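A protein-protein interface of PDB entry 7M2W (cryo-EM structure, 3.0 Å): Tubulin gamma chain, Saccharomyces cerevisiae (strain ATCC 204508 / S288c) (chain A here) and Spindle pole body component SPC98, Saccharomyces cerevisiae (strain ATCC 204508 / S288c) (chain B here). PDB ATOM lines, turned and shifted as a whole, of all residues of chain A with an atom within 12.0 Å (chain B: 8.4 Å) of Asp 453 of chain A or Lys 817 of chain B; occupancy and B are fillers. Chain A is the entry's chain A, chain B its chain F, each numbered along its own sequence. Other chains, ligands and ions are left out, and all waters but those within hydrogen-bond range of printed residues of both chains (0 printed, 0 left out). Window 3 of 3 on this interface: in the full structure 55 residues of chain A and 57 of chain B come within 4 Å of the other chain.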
ATOM      1  N   TRP A 347     -10.575  -3.798 -14.824  1.00  0.00           N
ATOM      2  CA  TRP A 347     -11.656  -3.383 -15.705  1.00  0.00           C
ATOM      3  C   TRP A 347     -11.681  -4.154 -17.019  1.00  0.00           C
ATOM      4  O   TRP A 347     -12.695  -4.116 -17.723  1.00  0.00           O
ATOM      5  CB  TRP A 347     -11.561  -1.882 -15.991  1.00  0.00           C
ATOM      6  CG  TRP A 347     -10.228  -1.427 -16.499  1.00  0.00           C
ATOM      7  CD1 TRP A 347      -9.223  -0.872 -15.768  1.00  0.00           C
ATOM      8  CD2 TRP A 347      -9.761  -1.478 -17.852  1.00  0.00           C
ATOM      9  NE1 TRP A 347      -8.156  -0.575 -16.578  1.00  0.00           N
ATOM     10  CE2 TRP A 347      -8.459  -0.940 -17.863  1.00  0.00           C
ATOM     11  CE3 TRP A 347     -10.314  -1.928 -19.054  1.00  0.00           C
ATOM     12  CZ2 TRP A 347      -7.703  -0.839 -19.027  1.00  0.00           C
ATOM     13  CZ3 TRP A 347      -9.560  -1.829 -20.209  1.00  0.00           C
ATOM     14  CH2 TRP A 347      -8.270  -1.288 -20.187  1.00  0.00           C
ATOM     15  N   SER A 349     -12.514  -7.048 -18.574  1.00  0.00           N
ATOM     16  CA  SER A 349     -13.294  -8.239 -18.261  1.00  0.00           C
ATOM     17  C   SER A 349     -13.043  -9.393 -19.220  1.00  0.00           C
ATOM     18  O   SER A 349     -13.741 -10.409 -19.135  1.00  0.00           O
ATOM     19  CB  SER A 349     -14.785  -7.900 -18.250  1.00  0.00           C
ATOM     20  OG  SER A 349     -15.346  -8.018 -19.545  1.00  0.00           O
ATOM     21  N   SER A 444     -10.540   3.338 -11.948  1.00  0.00           N
ATOM     22  CA  SER A 444     -11.434   4.441 -12.277  1.00  0.00           C
ATOM     23  C   SER A 444     -11.426   4.790 -13.759  1.00  0.00           C
ATOM     24  O   SER A 444     -12.244   5.614 -14.190  1.00  0.00           O
ATOM     25  CB  SER A 444     -11.065   5.676 -11.453  1.00  0.00           C
ATOM     26  OG  SER A 444     -11.260   5.439 -10.068  1.00  0.00           O
ATOM     27  N   LEU A 446     -12.543   3.129 -16.157  1.00  0.00           N
ATOM     28  CA  LEU A 446     -13.898   2.856 -16.615  1.00  0.00           C
ATOM     29  C   LEU A 446     -14.967   3.514 -15.754  1.00  0.00           C
ATOM     30  O   LEU A 446     -16.054   3.793 -16.266  1.00  0.00           O
ATOM     31  CB  LEU A 446     -14.157   1.348 -16.684  1.00  0.00           C
ATOM     32  CG  LEU A 446     -13.459   0.588 -17.811  1.00  0.00           C
ATOM     33  CD1 LEU A 446     -14.175  -0.727 -18.069  1.00  0.00           C
ATOM     34  CD2 LEU A 446     -13.397   1.426 -19.075  1.00  0.00           C
ATOM     35  N   ASP A 447     -14.697   3.770 -14.469  1.00  0.00           N
ATOM     36  CA  ASP A 447     -15.642   4.544 -13.666  1.00  0.00           C
ATOM     37  C   ASP A 447     -15.873   5.923 -14.262  1.00  0.00           C
ATOM     38  O   ASP A 447     -16.885   6.568 -13.965  1.00  0.00           O
ATOM     39  CB  ASP A 447     -15.149   4.667 -12.224  1.00  0.00           C
ATOM     40  CG  ASP A 447     -15.006   3.323 -11.539  1.00  0.00           C
ATOM     41  OD1 ASP A 447     -14.112   2.546 -11.928  1.00  0.00           O
ATOM     42  OD2 ASP A 447     -15.789   3.045 -10.605  1.00  0.00           O
ATOM     43  N   ASP A 448     -14.927   6.395 -15.077  1.00  0.00           N
ATOM     44  CA  ASP A 448     -15.130   7.600 -15.874  1.00  0.00           C
ATOM     45  C   ASP A 448     -16.489   7.610 -16.570  1.00  0.00           C
ATOM     46  O   ASP A 448     -17.156   8.651 -16.588  1.00  0.00           O
ATOM     47  CB  ASP A 448     -13.994   7.714 -16.903  1.00  0.00           C
ATOM     48  CG  ASP A 448     -13.986   9.043 -17.650  1.00  0.00           C
ATOM     49  OD1 ASP A 448     -15.055   9.517 -18.092  1.00  0.00           O
ATOM     50  OD2 ASP A 448     -12.889   9.619 -17.803  1.00  0.00           O
ATOM     51  N   VAL A 449     -16.928   6.479 -17.118  1.00  0.00           N
ATOM     52  CA  VAL A 449     -18.144   6.415 -17.915  1.00  0.00           C
ATOM     53  C   VAL A 449     -19.213   5.542 -17.265  1.00  0.00           C
ATOM     54  O   VAL A 449     -20.395   5.890 -17.291  1.00  0.00           O
ATOM     55  CB  VAL A 449     -17.835   5.934 -19.350  1.00  0.00           C
ATOM     56  CG1 VAL A 449     -17.306   4.508 -19.344  1.00  0.00           C
ATOM     57  CG2 VAL A 449     -19.074   6.048 -20.228  1.00  0.00           C
ATOM     58  N   LEU A 450     -18.823   4.402 -16.687  1.00  0.00           N
ATOM     59  CA  LEU A 450     -19.774   3.415 -16.188  1.00  0.00           C
ATOM     60  C   LEU A 450     -20.744   3.984 -15.163  1.00  0.00           C
ATOM     61  O   LEU A 450     -21.857   3.466 -15.031  1.00  0.00           O
ATOM     62  CB  LEU A 450     -19.024   2.223 -15.587  1.00  0.00           C
ATOM     63  CG  LEU A 450     -18.832   0.991 -16.479  1.00  0.00           C
ATOM     64  CD1 LEU A 450     -18.245   1.363 -17.831  1.00  0.00           C
ATOM     65  CD2 LEU A 450     -17.954  -0.038 -15.784  1.00  0.00           C
ATOM     66  N   VAL A 451     -20.353   5.033 -14.441  1.00  0.00           N
ATOM     67  CA  VAL A 451     -21.245   5.730 -13.527  1.00  0.00           C
ATOM     68  C   VAL A 451     -21.477   7.173 -13.954  1.00  0.00           C
ATOM     69  O   VAL A 451     -21.965   7.980 -13.162  1.00  0.00           O
ATOM     70  CB  VAL A 451     -20.727   5.664 -12.077  1.00  0.00           C
ATOM     71  CG1 VAL A 451     -20.772   4.233 -11.566  1.00  0.00           C
ATOM     72  CG2 VAL A 451     -19.321   6.222 -11.986  1.00  0.00           C
ATOM     73  N   ASP A 452     -21.139   7.515 -15.198  1.00  0.00           N
ATOM     74  CA  ASP A 452     -21.376   8.855 -15.737  1.00  0.00           C
ATOM     75  C   ASP A 452     -22.842   8.978 -16.159  1.00  0.00           C
ATOM     76  O   ASP A 452     -23.184   9.200 -17.322  1.00  0.00           O
ATOM     77  CB  ASP A 452     -20.432   9.135 -16.899  1.00  0.00           C
ATOM     78  CG  ASP A 452     -20.268  10.614 -17.173  1.00  0.00           C
ATOM     79  OD1 ASP A 452     -20.824  11.430 -16.408  1.00  0.00           O
ATOM     80  OD2 ASP A 452     -19.581  10.963 -18.156  1.00  0.00           O
ATOM     81  N   ASP A 453     -23.715   8.826 -15.169  1.00  0.00           N
ATOM     82  CA  ASP A 453     -25.153   8.853 -15.399  1.00  0.00           C
ATOM     83  C   ASP A 453     -25.678  10.284 -15.432  1.00  0.00           C
ATOM     84  O   ASP A 453     -24.935  11.240 -15.212  1.00  0.00           O
ATOM     85  CB  ASP A 453     -25.876   8.049 -14.318  1.00  0.00           C
ATOM     86  CG  ASP A 453     -25.254   6.685 -14.095  1.00  0.00           C
ATOM     87  OD1 ASP A 453     -25.057   5.949 -15.085  1.00  0.00           O
ATOM     88  OD2 ASP A 453     -24.959   6.352 -12.929  1.00  0.00           O
ATOM     89  N   LYS B 630     -16.144  10.058 -23.950  1.00  0.00           N
ATOM     90  CA  LYS B 630     -17.233   9.097 -24.083  1.00  0.00           C
ATOM     91  C   LYS B 630     -17.002   8.161 -25.261  1.00  0.00           C
ATOM     92  O   LYS B 630     -17.253   6.959 -25.153  1.00  0.00           O
ATOM     93  CB  LYS B 630     -18.579   9.812 -24.226  1.00  0.00           C
ATOM     94  CG  LYS B 630     -18.904  10.846 -23.149  1.00  0.00           C
ATOM     95  CD  LYS B 630     -18.867  10.277 -21.734  1.00  0.00           C
ATOM     96  CE  LYS B 630     -17.613  10.721 -20.985  1.00  0.00           C
ATOM     97  NZ  LYS B 630     -17.625  10.303 -19.556  1.00  0.00           N
ATOM     98  N   LEU B 637     -15.808  -0.391 -24.402  1.00  0.00           N
ATOM     99  CA  LEU B 637     -16.929  -1.298 -24.167  1.00  0.00           C
ATOM    100  C   LEU B 637     -17.175  -2.201 -25.372  1.00  0.00           C
ATOM    101  O   LEU B 637     -17.391  -3.413 -25.222  1.00  0.00           O
ATOM    102  CB  LEU B 637     -18.183  -0.494 -23.834  1.00  0.00           C
ATOM    103  CG  LEU B 637     -18.169   0.302 -22.527  1.00  0.00           C
ATOM    104  CD1 LEU B 637     -19.587   0.594 -22.067  1.00  0.00           C
ATOM    105  CD2 LEU B 637     -17.387  -0.425 -21.444  1.00  0.00           C
ATOM    106  N   PHE B 641     -17.014  -6.333 -25.574  1.00  0.00           N
ATOM    107  CA  PHE B 641     -18.028  -7.168 -26.213  1.00  0.00           C
ATOM    108  C   PHE B 641     -17.419  -8.061 -27.283  1.00  0.00           C
ATOM    109  O   PHE B 641     -17.632  -9.280 -27.285  1.00  0.00           O
ATOM    110  CB  PHE B 641     -19.118  -6.304 -26.841  1.00  0.00           C
ATOM    111  CG  PHE B 641     -20.256  -5.988 -25.928  1.00  0.00           C
ATOM    112  CD1 PHE B 641     -20.041  -5.703 -24.596  1.00  0.00           C
ATOM    113  CD2 PHE B 641     -21.553  -6.015 -26.402  1.00  0.00           C
ATOM    114  CE1 PHE B 641     -21.099  -5.412 -23.766  1.00  0.00           C
ATOM    115  CE2 PHE B 641     -22.611  -5.739 -25.571  1.00  0.00           C
ATOM    116  CZ  PHE B 641     -22.385  -5.435 -24.254  1.00  0.00           C
ATOM    117  N   PHE B 772     -26.485  -4.524 -29.221  1.00  0.00           N
ATOM    118  CA  PHE B 772     -25.509  -3.514 -28.834  1.00  0.00           C
ATOM    119  C   PHE B 772     -24.798  -2.948 -30.055  1.00  0.00           C
ATOM    120  O   PHE B 772     -24.525  -1.746 -30.122  1.00  0.00           O
ATOM    121  CB  PHE B 772     -24.509  -4.108 -27.845  1.00  0.00           C
ATOM    122  CG  PHE B 772     -23.381  -3.182 -27.480  1.00  0.00           C
ATOM    123  CD1 PHE B 772     -23.488  -2.344 -26.388  1.00  0.00           C
ATOM    124  CD2 PHE B 772     -22.205  -3.171 -28.210  1.00  0.00           C
ATOM    125  CE1 PHE B 772     -22.455  -1.498 -26.043  1.00  0.00           C
ATOM    126  CE2 PHE B 772     -21.168  -2.326 -27.870  1.00  0.00           C
ATOM    127  CZ  PHE B 772     -21.294  -1.490 -26.785  1.00  0.00           C
ATOM    128  N   ASN B 806     -26.273  11.789 -25.368  1.00  0.00           N
ATOM    129  CA  ASN B 806     -26.251  11.334 -23.982  1.00  0.00           C
ATOM    130  C   ASN B 806     -27.286  10.244 -23.726  1.00  0.00           C
ATOM    131  O   ASN B 806     -27.011   9.295 -22.980  1.00  0.00           O
ATOM    132  CB  ASN B 806     -26.477  12.511 -23.033  1.00  0.00           C
ATOM    133  CG  ASN B 806     -25.314  13.485 -23.024  1.00  0.00           C
ATOM    134  OD1 ASN B 806     -24.209  13.154 -23.449  1.00  0.00           O
ATOM    135  ND2 ASN B 806     -25.560  14.694 -22.533  1.00  0.00           N
ATOM    136  N   LEU B 809     -25.787   7.123 -25.065  1.00  0.00           N
ATOM    137  CA  LEU B 809     -24.700   6.636 -24.218  1.00  0.00           C
ATOM    138  C   LEU B 809     -25.234   5.941 -22.974  1.00  0.00           C
ATOM    139  O   LEU B 809     -24.729   4.885 -22.581  1.00  0.00           O
ATOM    140  CB  LEU B 809     -23.774   7.781 -23.811  1.00  0.00           C
ATOM    141  CG  LEU B 809     -22.996   8.547 -24.873  1.00  0.00           C
ATOM    142  CD1 LEU B 809     -22.692   9.934 -24.341  1.00  0.00           C
ATOM    143  CD2 LEU B 809     -21.720   7.820 -25.253  1.00  0.00           C
ATOM    144  N   LYS B 810     -26.242   6.528 -22.326  1.00  0.00           N
ATOM    145  CA  LYS B 810     -26.797   5.891 -21.135  1.00  0.00           C
ATOM    146  C   LYS B 810     -27.482   4.575 -21.485  1.00  0.00           C
ATOM    147  O   LYS B 810     -27.378   3.596 -20.735  1.00  0.00           O
ATOM    148  CB  LYS B 810     -27.758   6.844 -20.427  1.00  0.00           C
ATOM    149  CG  LYS B 810     -27.104   8.154 -20.017  1.00  0.00           C
ATOM    150  CD  LYS B 810     -28.104   9.132 -19.431  1.00  0.00           C
ATOM    151  CE  LYS B 810     -27.553  10.548 -19.453  1.00  0.00           C
ATOM    152  NZ  LYS B 810     -28.549  11.540 -18.973  1.00  0.00           N
ATOM    153  N   GLU B 811     -28.161   4.523 -22.633  1.00  0.00           N
ATOM    154  CA  GLU B 811     -28.730   3.263 -23.101  1.00  0.00           C
ATOM    155  C   GLU B 811     -27.640   2.223 -23.340  1.00  0.00           C
ATOM    156  O   GLU B 811     -27.791   1.051 -22.962  1.00  0.00           O
ATOM    157  CB  GLU B 811     -29.537   3.509 -24.376  1.00  0.00           C
ATOM    158  CG  GLU B 811     -29.905   2.260 -25.147  1.00  0.00           C
ATOM    159  CD  GLU B 811     -30.842   1.354 -24.379  1.00  0.00           C
ATOM    160  OE1 GLU B 811     -31.597   1.862 -23.523  1.00  0.00           O
ATOM    161  OE2 GLU B 811     -30.833   0.134 -24.638  1.00  0.00           O
ATOM    162  N   ILE B 812     -26.536   2.638 -23.965  1.00  0.00           N
ATOM    163  CA  ILE B 812     -25.426   1.732 -24.241  1.00  0.00           C
ATOM    164  C   ILE B 812     -24.835   1.198 -22.944  1.00  0.00           C
ATOM    165  O   ILE B 812     -24.520   0.009 -22.828  1.00  0.00           O
ATOM    166  CB  ILE B 812     -24.362   2.442 -25.098  1.00  0.00           C
ATOM    167  CG1 ILE B 812     -24.751   2.396 -26.575  1.00  0.00           C
ATOM    168  CG2 ILE B 812     -22.989   1.830 -24.884  1.00  0.00           C
ATOM    169  CD1 ILE B 812     -23.774   3.101 -27.480  1.00  0.00           C
ATOM    170  N   VAL B 813     -24.679   2.067 -21.944  1.00  0.00           N
ATOM    171  CA  VAL B 813     -24.076   1.636 -20.686  1.00  0.00           C
ATOM    172  C   VAL B 813     -25.015   0.699 -19.935  1.00  0.00           C
ATOM    173  O   VAL B 813     -24.576  -0.271 -19.304  1.00  0.00           O
ATOM    174  CB  VAL B 813     -23.678   2.855 -19.831  1.00  0.00           C
ATOM    175  CG1 VAL B 813     -23.118   2.406 -18.496  1.00  0.00           C
ATOM    176  CG2 VAL B 813     -22.651   3.698 -20.564  1.00  0.00           C
ATOM    177  N   SER B 814     -26.324   0.963 -19.999  1.00  0.00           N
ATOM    178  CA  SER B 814     -27.286   0.041 -19.404  1.00  0.00           C
ATOM    179  C   SER B 814     -27.202  -1.336 -20.052  1.00  0.00           C
ATOM    180  O   SER B 814     -27.174  -2.362 -19.357  1.00  0.00           O
ATOM    181  CB  SER B 814     -28.700   0.604 -19.528  1.00  0.00           C
ATOM    182  OG  SER B 814     -29.287   0.225 -20.761  1.00  0.00           O
ATOM    183  N   GLN B 815     -27.169  -1.377 -21.388  1.00  0.00           N
ATOM    184  CA  GLN B 815     -27.044  -2.656 -22.078  1.00  0.00           C
ATOM    185  C   GLN B 815     -25.723  -3.339 -21.744  1.00  0.00           C
ATOM    186  O   GLN B 815     -25.667  -4.568 -21.623  1.00  0.00           O
ATOM    187  CB  GLN B 815     -27.177  -2.457 -23.588  1.00  0.00           C
ATOM    188  CG  GLN B 815     -28.558  -2.024 -24.033  1.00  0.00           C
ATOM    189  CD  GLN B 815     -28.762  -2.169 -25.526  1.00  0.00           C
ATOM    190  OE1 GLN B 815     -27.912  -2.716 -26.230  1.00  0.00           O
ATOM    191  NE2 GLN B 815     -29.894  -1.681 -26.020  1.00  0.00           N
ATOM    192  N   TYR B 816     -24.653  -2.559 -21.590  1.00  0.00           N
ATOM    193  CA  TYR B 816     -23.354  -3.134 -21.260  1.00  0.00           C
ATOM    194  C   TYR B 816     -23.372  -3.761 -19.871  1.00  0.00           C
ATOM    195  O   TYR B 816     -22.803  -4.835 -19.655  1.00  0.00           O
ATOM    196  CB  TYR B 816     -22.269  -2.061 -21.359  1.00  0.00           C
ATOM    197  CG  TYR B 816     -20.943  -2.470 -20.766  1.00  0.00           C
ATOM    198  CD1 TYR B 816     -20.076  -3.290 -21.467  1.00  0.00           C
ATOM    199  CD2 TYR B 816     -20.555  -2.034 -19.508  1.00  0.00           C
ATOM    200  CE1 TYR B 816     -18.865  -3.671 -20.936  1.00  0.00           C
ATOM    201  CE2 TYR B 816     -19.343  -2.408 -18.968  1.00  0.00           C
ATOM    202  CZ  TYR B 816     -18.502  -3.227 -19.688  1.00  0.00           C
ATOM    203  OH  TYR B 816     -17.292  -3.606 -19.158  1.00  0.00           O
ATOM    204  N   LYS B 817     -24.044  -3.111 -18.919  1.00  0.00           N
ATOM    205  CA  LYS B 817     -24.173  -3.695 -17.587  1.00  0.00           C
ATOM    206  C   LYS B 817     -25.008  -4.969 -17.628  1.00  0.00           C
ATOM    207  O   LYS B 817     -24.660  -5.971 -16.984  1.00  0.00           O
ATOM    208  CB  LYS B 817     -24.797  -2.690 -16.621  1.00  0.00           C
ATOM    209  CG  LYS B 817     -23.951  -1.465 -16.333  1.00  0.00           C
ATOM    210  CD  LYS B 817     -24.816  -0.345 -15.777  1.00  0.00           C
ATOM    211  CE  LYS B 817     -23.987   0.867 -15.398  1.00  0.00           C
ATOM    212  NZ  LYS B 817     -24.847   2.047 -15.108  1.00  0.00           N
ATOM    213  N   ASN B 818     -26.132  -4.937 -18.351  1.00  0.00           N
ATOM    214  CA  ASN B 818     -26.931  -6.145 -18.536  1.00  0.00           C
ATOM    215  C   ASN B 818     -26.083  -7.290 -19.073  1.00  0.00           C
ATOM    216  O   ASN B 818     -26.115  -8.406 -18.537  1.00  0.00           O
ATOM    217  CB  ASN B 818     -28.099  -5.865 -19.482  1.00  0.00           C
ATOM    218  CG  ASN B 818     -29.233  -5.128 -18.806  1.00  0.00           C
ATOM    219  OD1 ASN B 818     -29.321  -5.095 -17.579  1.00  0.00           O
ATOM    220  ND2 ASN B 818     -30.113  -4.537 -19.604  1.00  0.00           N
ATOM    221  N   PHE B 819     -25.311  -7.027 -20.130  1.00  0.00           N
ATOM    222  CA  PHE B 819     -24.502  -8.076 -20.738  1.00  0.00           C
ATOM    223  C   PHE B 819     -23.416  -8.554 -19.787  1.00  0.00           C
ATOM    224  O   PHE B 819     -23.075  -9.737 -19.771  1.00  0.00           O
ATOM    225  CB  PHE B 819     -23.883  -7.585 -22.047  1.00  0.00           C
ATOM    226  CG  PHE B 819     -22.739  -8.434 -22.534  1.00  0.00           C
ATOM    227  CD1 PHE B 819     -22.966  -9.506 -23.376  1.00  0.00           C
ATOM    228  CD2 PHE B 819     -21.436  -8.160 -22.150  1.00  0.00           C
ATOM    229  CE1 PHE B 819     -21.920 -10.285 -23.823  1.00  0.00           C
ATOM    230  CE2 PHE B 819     -20.390  -8.934 -22.592  1.00  0.00           C
ATOM    231  CZ  PHE B 819     -20.632  -9.998 -23.429  1.00  0.00           C
ATOM    232  N   LYS B 820     -22.834  -7.642 -19.007  1.00  0.00           N
ATOM    233  CA  LYS B 820     -21.782  -8.047 -18.081  1.00  0.00           C
ATOM    234  C   LYS B 820     -22.330  -8.965 -16.999  1.00  0.00           C
ATOM    235  O   LYS B 820     -21.702  -9.971 -16.646  1.00  0.00           O
ATOM    236  CB  LYS B 820     -21.125  -6.815 -17.461  1.00  0.00           C
ATOM    237  CG  LYS B 820     -20.104  -6.143 -18.361  1.00  0.00           C
ATOM    238  CD  LYS B 820     -19.116  -7.150 -18.919  1.00  0.00           C
ATOM    239  CE  LYS B 820     -18.237  -7.714 -17.818  1.00  0.00           C
ATOM    240  NZ  LYS B 820     -17.662  -6.643 -16.962  1.00  0.00           N
ATOM    241  N   ASP B 821     -23.517  -8.653 -16.479  1.00  0.00           N
ATOM    242  CA  ASP B 821     -24.113  -9.530 -15.477  1.00  0.00           C
ATOM    243  C   ASP B 821     -24.518 -10.867 -16.086  1.00  0.00           C
ATOM    244  O   ASP B 821     -24.367 -11.918 -15.451  1.00  0.00           O
ATOM    245  CB  ASP B 821     -25.304  -8.840 -14.818  1.00  0.00           C
ATOM    246  CG  ASP B 821     -24.897  -7.994 -13.627  1.00  0.00           C
ATOM    247  OD1 ASP B 821     -24.362  -8.561 -12.651  1.00  0.00           O
ATOM    248  OD2 ASP B 821     -25.107  -6.764 -13.668  1.00  0.00           O
ATOM    249  N   ARG B 822     -25.009 -10.855 -17.327  1.00  0.00           N
ATOM    250  CA  ARG B 822     -25.358 -12.113 -17.982  1.00  0.00           C
ATOM    251  C   ARG B 822     -24.117 -12.948 -18.279  1.00  0.00           C
ATOM    252  O   ARG B 822     -24.160 -14.180 -18.208  1.00  0.00           O
ATOM    253  CB  ARG B 822     -26.151 -11.833 -19.257  1.00  0.00           C
ATOM    254  CG  ARG B 822     -27.561 -11.341 -18.986  1.00  0.00           C
ATOM    255  CD  ARG B 822     -28.444 -11.444 -20.215  1.00  0.00           C
ATOM    256  NE  ARG B 822     -29.844 -11.181 -19.894  1.00  0.00           N
ATOM    257  CZ  ARG B 822     -30.362  -9.966 -19.748  1.00  0.00           C
ATOM    258  NH1 ARG B 822     -29.597  -8.893 -19.893  1.00  0.00           N
ATOM    259  NH2 ARG B 822     -31.647  -9.824 -19.455  1.00  0.00           N
ATOM    260  N   LEU B 823     -22.998 -12.296 -18.594  1.00  0.00           N
ATOM    261  CA  LEU B 823     -21.754 -13.022 -18.818  1.00  0.00           C
ATOM    262  C   LEU B 823     -21.208 -13.586 -17.514  1.00  0.00           C
ATOM    263  O   LEU B 823     -20.609 -14.666 -17.503  1.00  0.00           O
ATOM    264  CB  LEU B 823     -20.725 -12.108 -19.485  1.00  0.00           C
ATOM    265  CG  LEU B 823     -19.273 -12.590 -19.504  1.00  0.00           C
ATOM    266  CD1 LEU B 823     -19.136 -13.869 -20.313  1.00  0.00           C
ATOM    267  CD2 LEU B 823     -18.354 -11.510 -20.047  1.00  0.00           C
ATOM    268  N   TYR B 824     -21.422 -12.884 -16.401  1.00  0.00           N
ATOM    269  CA  TYR B 824     -21.074 -13.450 -15.101  1.00  0.00           C
ATOM    270  C   TYR B 824     -21.931 -14.676 -14.801  1.00  0.00           C
ATOM    271  O   TYR B 824     -21.433 -15.694 -14.302  1.00  0.00           O
ATOM    272  CB  TYR B 824     -21.237 -12.392 -14.010  1.00  0.00           C
ATOM    273  CG  TYR B 824     -21.025 -12.908 -12.604  1.00  0.00           C
ATOM    274  CD1 TYR B 824     -19.747 -13.083 -12.092  1.00  0.00           C
ATOM    275  CD2 TYR B 824     -22.106 -13.211 -11.787  1.00  0.00           C
ATOM    276  CE1 TYR B 824     -19.550 -13.552 -10.809  1.00  0.00           C
ATOM    277  CE2 TYR B 824     -21.918 -13.680 -10.502  1.00  0.00           C
ATOM    278  CZ  TYR B 824     -20.640 -13.848 -10.018  1.00  0.00           C
ATOM    279  OH  TYR B 824     -20.451 -14.316  -8.737  1.00  0.00           O
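O of Leu 450 of chain A sits at hydrogen-bond distance from NZ of Lys 817 of chain B, 3.3 Å away. The side-chain amino group of Lys 630 of chain B is in salt-bridge range of the side-chain carboxylate of Asp 452 of chain A. The side-chain carboxylate (OD1) of Asp 448 of chain A is in salt-bridge range of the side-chain amino group (NZ) of Lys 630 of chain B (3.1 Å). The side-chain carboxylate of Asp 453 of chain A lies within salt-bridge range of the side-chain amino group of Lys 817 of chain B.
Among the printed residues, pairs that only touch across the chains: Ser 349 of chain A with Lys 820 of chain B (3.4 Å) and Leu 450 of chain A with Val 813 of chain B (3.8 Å).
Of the 21 printed residues of chain B, 4 touch a printed residue of chain A. Hydrophobic or aromatic side chains of chain B that line the printed part of chain A: Val 813.
Asp 453 of chain A touches just one residue of chain B: Lys 817 (3.9 Å). Lys 817 of chain B touches just these residues of chain A: Leu 450 (3.3 Å) and Asp 453 (3.9 Å). Lys 810 of chain B touches none of the printed residues of chain A. No residue of chain A comes within 4 Å of Asn 818 of chain B. Printed residues of chain B within 4 Å of Ser 349 of chain A: Lys 820. Of the printed residues of chain B, Asp 452 of chain A touches Lys 630 (2.5 Å). Of the printed residues of chain B, Asp 448 of chain A touches Lys 630. Printed residues of chain B within 4 Å of Leu 450 of chain A: Val 813 (3.8 Å) and Lys 817 (3.3 Å). Of the printed residues of chain A, Lys 630 of chain B touches Asp 448 (3.1 Å) and Asp 452 (2.5 Å). Leu 446 of chain A touches none of the printed residues of chain B. Leu 809 of chain B touches none of the printed residues of chain A. The nearest residue of chain A that does not touch Lys 817 of chain B is Val 451 of chain A (5.4 Å).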
